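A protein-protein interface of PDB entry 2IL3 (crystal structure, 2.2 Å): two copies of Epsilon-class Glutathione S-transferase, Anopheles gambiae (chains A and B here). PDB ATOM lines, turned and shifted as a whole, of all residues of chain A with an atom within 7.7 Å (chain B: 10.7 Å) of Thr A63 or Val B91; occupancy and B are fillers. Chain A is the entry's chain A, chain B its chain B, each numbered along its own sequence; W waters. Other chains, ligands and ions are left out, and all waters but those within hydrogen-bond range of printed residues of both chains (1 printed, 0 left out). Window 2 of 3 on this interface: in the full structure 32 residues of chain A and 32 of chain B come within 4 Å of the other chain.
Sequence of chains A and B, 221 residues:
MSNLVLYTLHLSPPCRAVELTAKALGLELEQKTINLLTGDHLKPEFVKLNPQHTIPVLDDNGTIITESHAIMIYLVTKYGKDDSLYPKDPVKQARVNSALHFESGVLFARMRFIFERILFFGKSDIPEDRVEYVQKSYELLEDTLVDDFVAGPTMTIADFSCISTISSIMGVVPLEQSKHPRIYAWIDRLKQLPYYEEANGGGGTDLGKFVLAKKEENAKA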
ATOM      1  N   LEU A   4      33.054  -9.474 -24.448  1.00  0.00           N
ATOM      2  CA  LEU A   4      32.472  -9.741 -23.135  1.00  0.00           C
ATOM      3  C   LEU A   4      32.754 -11.182 -22.644  1.00  0.00           C
ATOM      4  O   LEU A   4      32.656 -12.164 -23.414  1.00  0.00           O
ATOM      5  CB  LEU A   4      30.958  -9.473 -23.155  1.00  0.00           C
ATOM      6  CG  LEU A   4      30.398  -8.229 -23.866  1.00  0.00           C
ATOM      7  CD1 LEU A   4      28.928  -8.435 -24.309  1.00  0.00           C
ATOM      8  CD2 LEU A   4      30.487  -7.044 -22.995  1.00  0.00           C
ATOM      9  N   VAL A   5      33.109 -11.301 -21.368  1.00  0.00           N
ATOM     10  CA  VAL A   5      33.299 -12.594 -20.742  1.00  0.00           C
ATOM     11  C   VAL A   5      32.238 -12.916 -19.686  1.00  0.00           C
ATOM     12  O   VAL A   5      31.936 -12.120 -18.795  1.00  0.00           O
ATOM     13  CB  VAL A   5      34.689 -12.685 -20.088  1.00  0.00           C
ATOM     14  CG1 VAL A   5      34.690 -13.585 -18.772  1.00  0.00           C
ATOM     15  CG2 VAL A   5      35.720 -13.196 -21.123  1.00  0.00           C
ATOM     16  N   LEU A  49      36.477 -11.662  -7.561  1.00  0.00           N
ATOM     17  CA  LEU A  49      35.540 -11.123  -8.514  1.00  0.00           C
ATOM     18  C   LEU A  49      34.161 -10.951  -7.884  1.00  0.00           C
ATOM     19  O   LEU A  49      33.383 -10.098  -8.291  1.00  0.00           O
ATOM     20  CB  LEU A  49      35.347 -12.101  -9.644  1.00  0.00           C
ATOM     21  CG  LEU A  49      36.306 -12.255 -10.807  1.00  0.00           C
ATOM     22  CD1 LEU A  49      35.818 -13.461 -11.571  1.00  0.00           C
ATOM     23  CD2 LEU A  49      36.357 -11.018 -11.684  1.00  0.00           C
ATOM     24  N   VAL A  57      29.067 -14.198 -13.619  1.00  0.00           N
ATOM     25  CA  VAL A  57      29.757 -12.958 -13.478  1.00  0.00           C
ATOM     26  C   VAL A  57      30.106 -12.422 -14.829  1.00  0.00           C
ATOM     27  O   VAL A  57      30.720 -13.087 -15.580  1.00  0.00           O
ATOM     28  CB  VAL A  57      31.038 -13.083 -12.562  1.00  0.00           C
ATOM     29  CG1 VAL A  57      31.917 -11.825 -12.643  1.00  0.00           C
ATOM     30  CG2 VAL A  57      30.635 -13.283 -11.110  1.00  0.00           C
ATOM     31  N   LEU A  58      29.740 -11.186 -15.112  1.00  0.00           N
ATOM     32  CA  LEU A  58      30.185 -10.491 -16.290  1.00  0.00           C
ATOM     33  C   LEU A  58      31.475  -9.681 -16.115  1.00  0.00           C
ATOM     34  O   LEU A  58      31.597  -8.968 -15.160  1.00  0.00           O
ATOM     35  CB  LEU A  58      29.105  -9.568 -16.877  1.00  0.00           C
ATOM     36  CG  LEU A  58      29.363  -9.154 -18.362  1.00  0.00           C
ATOM     37  CD1 LEU A  58      29.029 -10.237 -19.351  1.00  0.00           C
ATOM     38  CD2 LEU A  58      28.620  -7.859 -18.711  1.00  0.00           C
ATOM     39  N   ASP A  59      32.395  -9.805 -17.086  1.00  0.00           N
ATOM     40  CA  ASP A  59      33.570  -9.008 -17.209  1.00  0.00           C
ATOM     41  C   ASP A  59      33.557  -8.351 -18.597  1.00  0.00           C
ATOM     42  O   ASP A  59      33.672  -8.983 -19.611  1.00  0.00           O
ATOM     43  CB  ASP A  59      34.825  -9.864 -16.958  1.00  0.00           C
ATOM     44  CG  ASP A  59      36.189  -9.144 -17.324  1.00  0.00           C
ATOM     45  OD1 ASP A  59      36.241  -7.951 -17.753  1.00  0.00           O
ATOM     46  OD2 ASP A  59      37.237  -9.830 -17.170  1.00  0.00           O
ATOM     47  N   ASP A  60      33.379  -7.058 -18.626  1.00  0.00           N
ATOM     48  CA  ASP A  60      33.329  -6.314 -19.889  1.00  0.00           C
ATOM     49  C   ASP A  60      34.509  -5.341 -19.940  1.00  0.00           C
ATOM     50  O   ASP A  60      34.297  -4.161 -19.826  1.00  0.00           O
ATOM     51  CB  ASP A  60      31.996  -5.536 -19.970  1.00  0.00           C
ATOM     52  CG  ASP A  60      31.789  -4.841 -21.314  1.00  0.00           C
ATOM     53  OD1 ASP A  60      30.718  -4.275 -21.535  1.00  0.00           O
ATOM     54  OD2 ASP A  60      32.666  -4.893 -22.196  1.00  0.00           O
ATOM     55  N   ASN A  61      35.745  -5.823 -20.115  1.00  0.00           N
ATOM     56  CA  ASN A  61      36.949  -5.005 -20.312  1.00  0.00           C
ATOM     57  C   ASN A  61      37.092  -4.137 -19.113  1.00  0.00           C
ATOM     58  O   ASN A  61      37.045  -2.929 -19.269  1.00  0.00           O
ATOM     59  CB  ASN A  61      36.881  -3.975 -21.477  1.00  0.00           C
ATOM     60  CG  ASN A  61      36.161  -4.480 -22.715  1.00  0.00           C
ATOM     61  OD1 ASN A  61      35.157  -5.166 -22.618  1.00  0.00           O
ATOM     62  ND2 ASN A  61      36.667  -4.097 -23.918  1.00  0.00           N
ATOM     63  N   GLY A  62      37.223  -4.714 -17.939  1.00  0.00           N
ATOM     64  CA  GLY A  62      37.440  -3.948 -16.784  1.00  0.00           C
ATOM     65  C   GLY A  62      36.240  -4.035 -15.878  1.00  0.00           C
ATOM     66  O   GLY A  62      36.421  -4.242 -14.669  1.00  0.00           O
ATOM     67  N   THR A  63      35.033  -3.820 -16.417  1.00  0.00           N
ATOM     68  CA  THR A  63      33.813  -3.741 -15.577  1.00  0.00           C
ATOM     69  C   THR A  63      33.318  -5.124 -15.209  1.00  0.00           C
ATOM     70  O   THR A  63      33.074  -5.941 -16.101  1.00  0.00           O
ATOM     71  CB  THR A  63      32.604  -3.019 -16.277  1.00  0.00           C
ATOM     72  OG1 THR A  63      33.006  -1.759 -16.833  1.00  0.00           O
ATOM     73  CG2 THR A  63      31.415  -2.815 -15.285  1.00  0.00           C
ATOM     74  N   ILE A  64      33.132  -5.371 -13.908  1.00  0.00           N
ATOM     75  CA  ILE A  64      32.677  -6.635 -13.410  1.00  0.00           C
ATOM     76  C   ILE A  64      31.262  -6.445 -12.836  1.00  0.00           C
ATOM     77  O   ILE A  64      31.007  -5.538 -12.019  1.00  0.00           O
ATOM     78  CB  ILE A  64      33.698  -7.263 -12.462  1.00  0.00           C
ATOM     79  CG1 ILE A  64      34.722  -8.084 -13.256  1.00  0.00           C
ATOM     80  CG2 ILE A  64      33.113  -8.294 -11.554  1.00  0.00           C
ATOM     81  CD1 ILE A  64      35.914  -7.323 -13.645  1.00  0.00           C
ATOM     82  N   ILE A  65      30.327  -7.270 -13.327  1.00  0.00           N
ATOM     83  CA  ILE A  65      28.962  -7.195 -12.857  1.00  0.00           C
ATOM     84  C   ILE A  65      28.596  -8.574 -12.395  1.00  0.00           C
ATOM     85  O   ILE A  65      28.740  -9.511 -13.133  1.00  0.00           O
ATOM     86  CB  ILE A  65      27.962  -6.731 -13.971  1.00  0.00           C
ATOM     87  CG1 ILE A  65      28.402  -5.418 -14.623  1.00  0.00           C
ATOM     88  CG2 ILE A  65      26.491  -6.655 -13.409  1.00  0.00           C
ATOM     89  CD1 ILE A  65      28.011  -5.392 -16.032  1.00  0.00           C
ATOM     90  N   THR A  66      28.152  -8.679 -11.165  1.00  0.00           N
ATOM     91  CA  THR A  66      27.689  -9.889 -10.585  1.00  0.00           C
ATOM     92  C   THR A  66      26.115  -9.947 -10.828  1.00  0.00           C
ATOM     93  O   THR A  66      25.469  -8.998 -11.374  1.00  0.00           O
ATOM     94  CB  THR A  66      28.344 -10.098  -9.079  1.00  0.00           C
ATOM     95  OG1 THR A  66      27.757  -9.286  -8.048  1.00  0.00           O
ATOM     96  CG2 THR A  66      29.834  -9.730  -9.056  1.00  0.00           C
ATOM     97  N   TYR A  74      22.173  -4.285 -17.776  1.00  0.00           N
ATOM     98  CA  TYR A  74      23.376  -3.637 -18.322  1.00  0.00           C
ATOM     99  C   TYR A  74      23.680  -4.018 -19.754  1.00  0.00           C
ATOM    100  O   TYR A  74      24.147  -3.182 -20.594  1.00  0.00           O
ATOM    101  CB  TYR A  74      24.546  -3.943 -17.372  1.00  0.00           C
ATOM    102  CG  TYR A  74      25.893  -3.575 -17.895  1.00  0.00           C
ATOM    103  CD1 TYR A  74      26.518  -2.357 -17.508  1.00  0.00           C
ATOM    104  CD2 TYR A  74      26.578  -4.427 -18.825  1.00  0.00           C
ATOM    105  CE1 TYR A  74      27.786  -1.996 -18.029  1.00  0.00           C
ATOM    106  CE2 TYR A  74      27.849  -4.076 -19.329  1.00  0.00           C
ATOM    107  CZ  TYR A  74      28.446  -2.869 -18.920  1.00  0.00           C
ATOM    108  OH  TYR A  74      29.725  -2.555 -19.390  1.00  0.00           O
ATOM    109  N   LYS A  78      23.562  -1.170 -22.548  1.00  0.00           N
ATOM    110  CA  LYS A  78      24.717  -0.827 -23.342  1.00  0.00           C
ATOM    111  C   LYS A  78      24.558  -1.225 -24.795  1.00  0.00           C
ATOM    112  O   LYS A  78      25.060  -0.498 -25.716  1.00  0.00           O
ATOM    113  CB  LYS A  78      25.980  -1.454 -22.763  1.00  0.00           C
ATOM    114  CG  LYS A  78      27.320  -0.842 -23.270  1.00  0.00           C
ATOM    115  CD  LYS A  78      28.263  -0.534 -22.094  1.00  0.00           C
ATOM    116  CE  LYS A  78      29.697  -1.163 -22.223  1.00  0.00           C
ATOM    117  NZ  LYS A  78      30.693  -0.418 -23.086  1.00  0.00           N
ATOM    118  N   ASP B  83      20.392  11.416  -8.928  1.00  0.00           N
ATOM    119  CA  ASP B  83      20.504   9.947  -9.019  1.00  0.00           C
ATOM    120  C   ASP B  83      21.309   9.433  -7.771  1.00  0.00           C
ATOM    121  O   ASP B  83      22.165   8.508  -7.829  1.00  0.00           O
ATOM    122  CB  ASP B  83      21.158   9.517 -10.377  1.00  0.00           C
ATOM    123  CG  ASP B  83      22.683   9.753 -10.410  1.00  0.00           C
ATOM    124  OD1 ASP B  83      23.121  10.519  -9.527  1.00  0.00           O
ATOM    125  OD2 ASP B  83      23.473   9.164 -11.249  1.00  0.00           O
ATOM    126  N   TYR B  86      19.666   5.975  -6.724  1.00  0.00           N
ATOM    127  CA  TYR B  86      19.712   4.993  -7.724  1.00  0.00           C
ATOM    128  C   TYR B  86      20.576   5.557  -8.873  1.00  0.00           C
ATOM    129  O   TYR B  86      20.025   6.173  -9.782  1.00  0.00           O
ATOM    130  CB  TYR B  86      18.295   4.744  -8.225  1.00  0.00           C
ATOM    131  CG  TYR B  86      18.154   3.563  -9.155  1.00  0.00           C
ATOM    132  CD1 TYR B  86      18.330   2.265  -8.691  1.00  0.00           C
ATOM    133  CD2 TYR B  86      17.817   3.748 -10.481  1.00  0.00           C
ATOM    134  CE1 TYR B  86      18.235   1.178  -9.553  1.00  0.00           C
ATOM    135  CE2 TYR B  86      17.738   2.663 -11.350  1.00  0.00           C
ATOM    136  CZ  TYR B  86      17.940   1.371 -10.864  1.00  0.00           C
ATOM    137  OH  TYR B  86      17.788   0.286 -11.704  1.00  0.00           O
ATOM    138  N   PRO B  87      21.914   5.266  -8.886  1.00  0.00           N
ATOM    139  CA  PRO B  87      22.756   5.887  -9.947  1.00  0.00           C
ATOM    140  C   PRO B  87      22.259   5.606 -11.373  1.00  0.00           C
ATOM    141  O   PRO B  87      21.757   4.547 -11.646  1.00  0.00           O
ATOM    142  CB  PRO B  87      24.145   5.282  -9.745  1.00  0.00           C
ATOM    143  CG  PRO B  87      24.079   4.499  -8.414  1.00  0.00           C
ATOM    144  CD  PRO B  87      22.642   4.308  -8.023  1.00  0.00           C
ATOM    145  N   LYS B  88      22.431   6.588 -12.264  1.00  0.00           N
ATOM    146  CA  LYS B  88      22.119   6.485 -13.696  1.00  0.00           C
ATOM    147  C   LYS B  88      23.255   5.933 -14.549  1.00  0.00           C
ATOM    148  O   LYS B  88      22.970   5.253 -15.490  1.00  0.00           O
ATOM    149  CB  LYS B  88      21.566   7.818 -14.239  1.00  0.00           C
ATOM    150  CG  LYS B  88      20.129   8.049 -13.807  1.00  0.00           C
ATOM    151  CD  LYS B  88      19.485   9.380 -14.331  1.00  0.00           C
ATOM    152  CE  LYS B  88      18.080   9.624 -13.719  1.00  0.00           C
ATOM    153  NZ  LYS B  88      18.095   9.812 -12.176  1.00  0.00           N
ATOM    154  N   ASP B  89      24.524   6.194 -14.203  1.00  0.00           N
ATOM    155  CA  ASP B  89      25.657   5.438 -14.684  1.00  0.00           C
ATOM    156  C   ASP B  89      25.428   3.899 -14.701  1.00  0.00           C
ATOM    157  O   ASP B  89      25.255   3.286 -13.620  1.00  0.00           O
ATOM    158  CB  ASP B  89      26.880   5.671 -13.790  1.00  0.00           C
ATOM    159  CG  ASP B  89      28.116   4.906 -14.286  1.00  0.00           C
ATOM    160  OD1 ASP B  89      28.490   3.878 -13.678  1.00  0.00           O
ATOM    161  OD2 ASP B  89      28.679   5.274 -15.336  1.00  0.00           O
ATOM    162  N   PRO B  90      25.531   3.273 -15.902  1.00  0.00           N
ATOM    163  CA  PRO B  90      25.368   1.809 -16.104  1.00  0.00           C
ATOM    164  C   PRO B  90      26.094   0.904 -15.102  1.00  0.00           C
ATOM    165  O   PRO B  90      25.455  -0.026 -14.515  1.00  0.00           O
ATOM    166  CB  PRO B  90      25.842   1.609 -17.556  1.00  0.00           C
ATOM    167  CG  PRO B  90      25.298   2.899 -18.214  1.00  0.00           C
ATOM    168  CD  PRO B  90      25.718   3.968 -17.208  1.00  0.00           C
ATOM    169  N   VAL B  91      27.377   1.204 -14.856  1.00  0.00           N
ATOM    170  CA  VAL B  91      28.191   0.443 -13.868  1.00  0.00           C
ATOM    171  C   VAL B  91      27.799   0.617 -12.400  1.00  0.00           C
ATOM    172  O   VAL B  91      27.751  -0.345 -11.628  1.00  0.00           O
ATOM    173  CB  VAL B  91      29.692   0.851 -13.970  1.00  0.00           C
ATOM    174  CG1 VAL B  91      30.589  -0.179 -13.237  1.00  0.00           C
ATOM    175  CG2 VAL B  91      30.100   1.095 -15.466  1.00  0.00           C
ATOM    176  N   LYS B  92      27.647   1.853 -11.944  1.00  0.00           N
ATOM    177  CA  LYS B  92      27.166   2.013 -10.579  1.00  0.00           C
ATOM    178  C   LYS B  92      25.739   1.657 -10.443  1.00  0.00           C
ATOM    179  O   LYS B  92      25.370   1.201  -9.363  1.00  0.00           O
ATOM    180  CB  LYS B  92      27.371   3.431 -10.091  1.00  0.00           C
ATOM    181  CG  LYS B  92      28.756   3.938 -10.409  1.00  0.00           C
ATOM    182  CD  LYS B  92      28.850   5.410 -10.128  1.00  0.00           C
ATOM    183  CE  LYS B  92      30.318   5.822 -10.304  1.00  0.00           C
ATOM    184  NZ  LYS B  92      30.463   7.323 -10.545  1.00  0.00           N
ATOM    185  N   GLN B  93      24.896   1.913 -11.461  1.00  0.00           N
ATOM    186  CA  GLN B  93      23.580   1.272 -11.474  1.00  0.00           C
ATOM    187  C   GLN B  93      23.585  -0.274 -11.288  1.00  0.00           C
ATOM    188  O   GLN B  93      22.754  -0.811 -10.569  1.00  0.00           O
ATOM    189  CB  GLN B  93      22.730   1.617 -12.692  1.00  0.00           C
ATOM    190  CG  GLN B  93      21.300   1.328 -12.486  1.00  0.00           C
ATOM    191  CD  GLN B  93      20.529   1.684 -13.698  1.00  0.00           C
ATOM    192  OE1 GLN B  93      20.367   0.884 -14.588  1.00  0.00           O
ATOM    193  NE2 GLN B  93      20.138   2.933 -13.799  1.00  0.00           N
ATOM    194  N   ALA B  94      24.492  -0.967 -11.942  1.00  0.00           N
ATOM    195  CA  ALA B  94      24.516  -2.427 -11.948  1.00  0.00           C
ATOM    196  C   ALA B  94      24.865  -2.898 -10.536  1.00  0.00           C
ATOM    197  O   ALA B  94      24.236  -3.853 -10.065  1.00  0.00           O
ATOM    198  CB  ALA B  94      25.538  -2.911 -12.952  1.00  0.00           C
ATOM    199  N   ARG B  95      25.819  -2.226  -9.854  1.00  0.00           N
ATOM    200  CA  ARG B  95      26.163  -2.554  -8.494  1.00  0.00           C
ATOM    201  C   ARG B  95      24.921  -2.485  -7.607  1.00  0.00           C
ATOM    202  O   ARG B  95      24.618  -3.371  -6.866  1.00  0.00           O
ATOM    203  CB  ARG B  95      27.263  -1.575  -7.989  1.00  0.00           C
ATOM    204  CG  ARG B  95      27.738  -1.949  -6.629  1.00  0.00           C
ATOM    205  CD  ARG B  95      29.141  -1.547  -6.365  1.00  0.00           C
ATOM    206  NE  ARG B  95      29.526  -1.871  -4.987  1.00  0.00           N
ATOM    207  CZ  ARG B  95      30.558  -1.310  -4.366  1.00  0.00           C
ATOM    208  NH1 ARG B  95      30.845  -1.631  -3.109  1.00  0.00           N
ATOM    209  NH2 ARG B  95      31.300  -0.424  -4.994  1.00  0.00           N
ATOM    210  N   VAL B  96      24.122  -1.441  -7.755  1.00  0.00           N
ATOM    211  CA  VAL B  96      22.860  -1.319  -7.038  1.00  0.00           C
ATOM    212  C   VAL B  96      21.814  -2.331  -7.493  1.00  0.00           C
ATOM    213  O   VAL B  96      21.003  -2.788  -6.706  1.00  0.00           O
ATOM    214  CB  VAL B  96      22.332   0.093  -7.313  1.00  0.00           C
ATOM    215  CG1 VAL B  96      20.937   0.349  -6.711  1.00  0.00           C
ATOM    216  CG2 VAL B  96      23.388   1.127  -6.729  1.00  0.00           C
ATOM    217  N   ASN B  97      21.765  -2.687  -8.758  1.00  0.00           N
ATOM    218  CA  ASN B  97      20.690  -3.629  -9.122  1.00  0.00           C
ATOM    219  C   ASN B  97      21.127  -4.993  -8.635  1.00  0.00           C
ATOM    220  O   ASN B  97      20.272  -5.777  -8.380  1.00  0.00           O
ATOM    221  CB  ASN B  97      20.510  -3.806 -10.597  1.00  0.00           C
ATOM    222  CG  ASN B  97      19.864  -2.677 -11.263  1.00  0.00           C
ATOM    223  OD1 ASN B  97      20.288  -2.315 -12.396  1.00  0.00           O
ATOM    224  ND2 ASN B  97      18.824  -2.111 -10.646  1.00  0.00           N
ATOM    225  N   SER B  98      22.443  -5.252  -8.498  1.00  0.00           N
ATOM    226  CA  SER B  98      22.924  -6.531  -7.874  1.00  0.00           C
ATOM    227  C   SER B  98      22.586  -6.667  -6.398  1.00  0.00           C
ATOM    228  O   SER B  98      22.253  -7.705  -5.982  1.00  0.00           O
ATOM    229  CB  SER B  98      24.472  -6.749  -8.015  1.00  0.00           C
ATOM    230  OG  SER B  98      24.886  -6.778  -9.340  1.00  0.00           O
ATOM    231  N   ALA B  99      22.780  -5.618  -5.610  1.00  0.00           N
ATOM    232  CA  ALA B  99      22.388  -5.589  -4.190  1.00  0.00           C
ATOM    233  C   ALA B  99      20.875  -5.742  -3.984  1.00  0.00           C
ATOM    234  O   ALA B  99      20.342  -6.534  -3.108  1.00  0.00           O
ATOM    235  CB  ALA B  99      22.962  -4.280  -3.550  1.00  0.00           C
ATOM    236  N   VAL B 150      25.688  -0.498   1.077  1.00  0.00           N
ATOM    237  CA  VAL B 150      25.697  -1.869   0.548  1.00  0.00           C
ATOM    238  C   VAL B 150      26.158  -1.986  -0.893  1.00  0.00           C
ATOM    239  O   VAL B 150      26.668  -3.104  -1.369  1.00  0.00           O
ATOM    240  CB  VAL B 150      24.383  -2.643   0.815  1.00  0.00           C
ATOM    241  CG1 VAL B 150      23.282  -2.285  -0.195  1.00  0.00           C
ATOM    242  CG2 VAL B 150      24.700  -4.137   0.759  1.00  0.00           C
ATOM    243  N   ALA B 151      25.963  -0.861  -1.595  1.00  0.00           N
ATOM    244  CA  ALA B 151      26.169  -0.842  -3.002  1.00  0.00           C
ATOM    245  C   ALA B 151      27.223   0.206  -3.294  1.00  0.00           C
ATOM    246  O   ALA B 151      27.366   0.638  -4.449  1.00  0.00           O
ATOM    247  CB  ALA B 151      24.859  -0.526  -3.723  1.00  0.00           C
ATOM    248  N   GLY B 152      27.944   0.619  -2.240  1.00  0.00           N
ATOM    249  CA  GLY B 152      29.137   1.442  -2.372  1.00  0.00           C
ATOM    250  C   GLY B 152      29.266   2.593  -1.419  1.00  0.00           C
ATOM    251  O   GLY B 152      28.695   2.567  -0.320  1.00  0.00           O
ATOM    252  N   PRO B 153      30.008   3.647  -1.836  1.00  0.00           N
ATOM    253  CA  PRO B 153      30.387   4.708  -0.888  1.00  0.00           C
ATOM    254  C   PRO B 153      29.177   5.483  -0.332  1.00  0.00           C
ATOM    255  O   PRO B 153      29.228   6.102   0.730  1.00  0.00           O
ATOM    256  CB  PRO B 153      31.332   5.586  -1.719  1.00  0.00           C
ATOM    257  CG  PRO B 153      31.823   4.645  -2.749  1.00  0.00           C
ATOM    258  CD  PRO B 153      30.609   3.900  -3.152  1.00  0.00           C
ATOM    259  N   THR B 156      22.046   4.004  -1.111  1.00  0.00           N
ATOM    260  CA  THR B 156      21.032   3.837  -2.184  1.00  0.00           C
ATOM    261  C   THR B 156      19.739   3.218  -1.641  1.00  0.00           C
ATOM    262  O   THR B 156      19.717   2.821  -0.524  1.00  0.00           O
ATOM    263  CB  THR B 156      21.595   2.943  -3.407  1.00  0.00           C
ATOM    264  OG1 THR B 156      21.922   1.634  -2.976  1.00  0.00           O
ATOM    265  CG2 THR B 156      22.842   3.496  -3.945  1.00  0.00           C
HETATM  266  O   HOH W   1      28.784  -3.528 -11.120  1.00  0.00           O
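Water W1 lies within hydrogen-bond range of O of Ile A64 (3.1 Å), O of Val B91 (3.4 Å) and N of Arg B95 (3.5 Å).
O of Ile A65 is in hydrogen-bond range of N of Leu A58, at 2.8 Å.
The side-chain carboxylate (OD1) of Asp A60 lies within hydrogen-bond range of the side-chain hydroxyl (OH) of Tyr A74 (2.9 Å).
The side-chain carboxylate (OD1) of Asp B89 sits at hydrogen-bond distance from the backbone NH (N) of Val B91.
The backbone carbonyl oxygen (O) of Ala B94 lies within hydrogen-bond range of the side-chain hydroxyl (OG) of Ser B98, at 3.1 Å.
The backbone carbonyl oxygen of Thr A66 lies within hydrogen-bond range of the side-chain hydroxyl of Ser B98 (3.1 Å).
Hydrophobic or aromatic side chains of chain A within 4 Å of the printed part of chain B: Ile A65 and Tyr A74.
Printed residues of chain B that touch a printed residue of chain A: Pro B90, Val B91, Ala B94 and Ser B98.
Among the printed residues, no Asp or Glu carboxylate lies within 4 Å of a Lys or Arg side-chain nitrogen of the other chain.
Asp A60 touches none of the printed residues of chain B.
No residue of chain B comes within 4 Å of Gly A62.
Ile A65 touches one residue of chain B.
Printed residues of chain A within 4 Å of Pro B90: Tyr A74 (3.9 Å).
Of the printed residues of chain B, Thr A66 touches Ser B98 (3.1 Å).
Of the printed residues of chain B, Tyr A74 touches Pro B90.
Of the printed residues of chain A, Ser B98 touches Thr A66 (3.1 Å).
Printed residues of chain A within 4 Å of Ala B94: Ile A65.
The nearest residue of chain B that does not touch Thr A63 is Ala B94 (6.3 Å).
The nearest residue of chain A that does not touch Val B91 is Tyr A74 (4.5 Å).
No position is printed for both chains.
Of the 4 pairs that touch across the chains among the printed residues, none has its exchanged pair printed and touching as well.
Among the printed residues, pairs that only touch across the chains: Thr A63 with Val B91 (3.4 Å), Ile A65 with Ala B94 (3.9 Å) and Tyr A74 with Pro B90 (3.9 Å).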
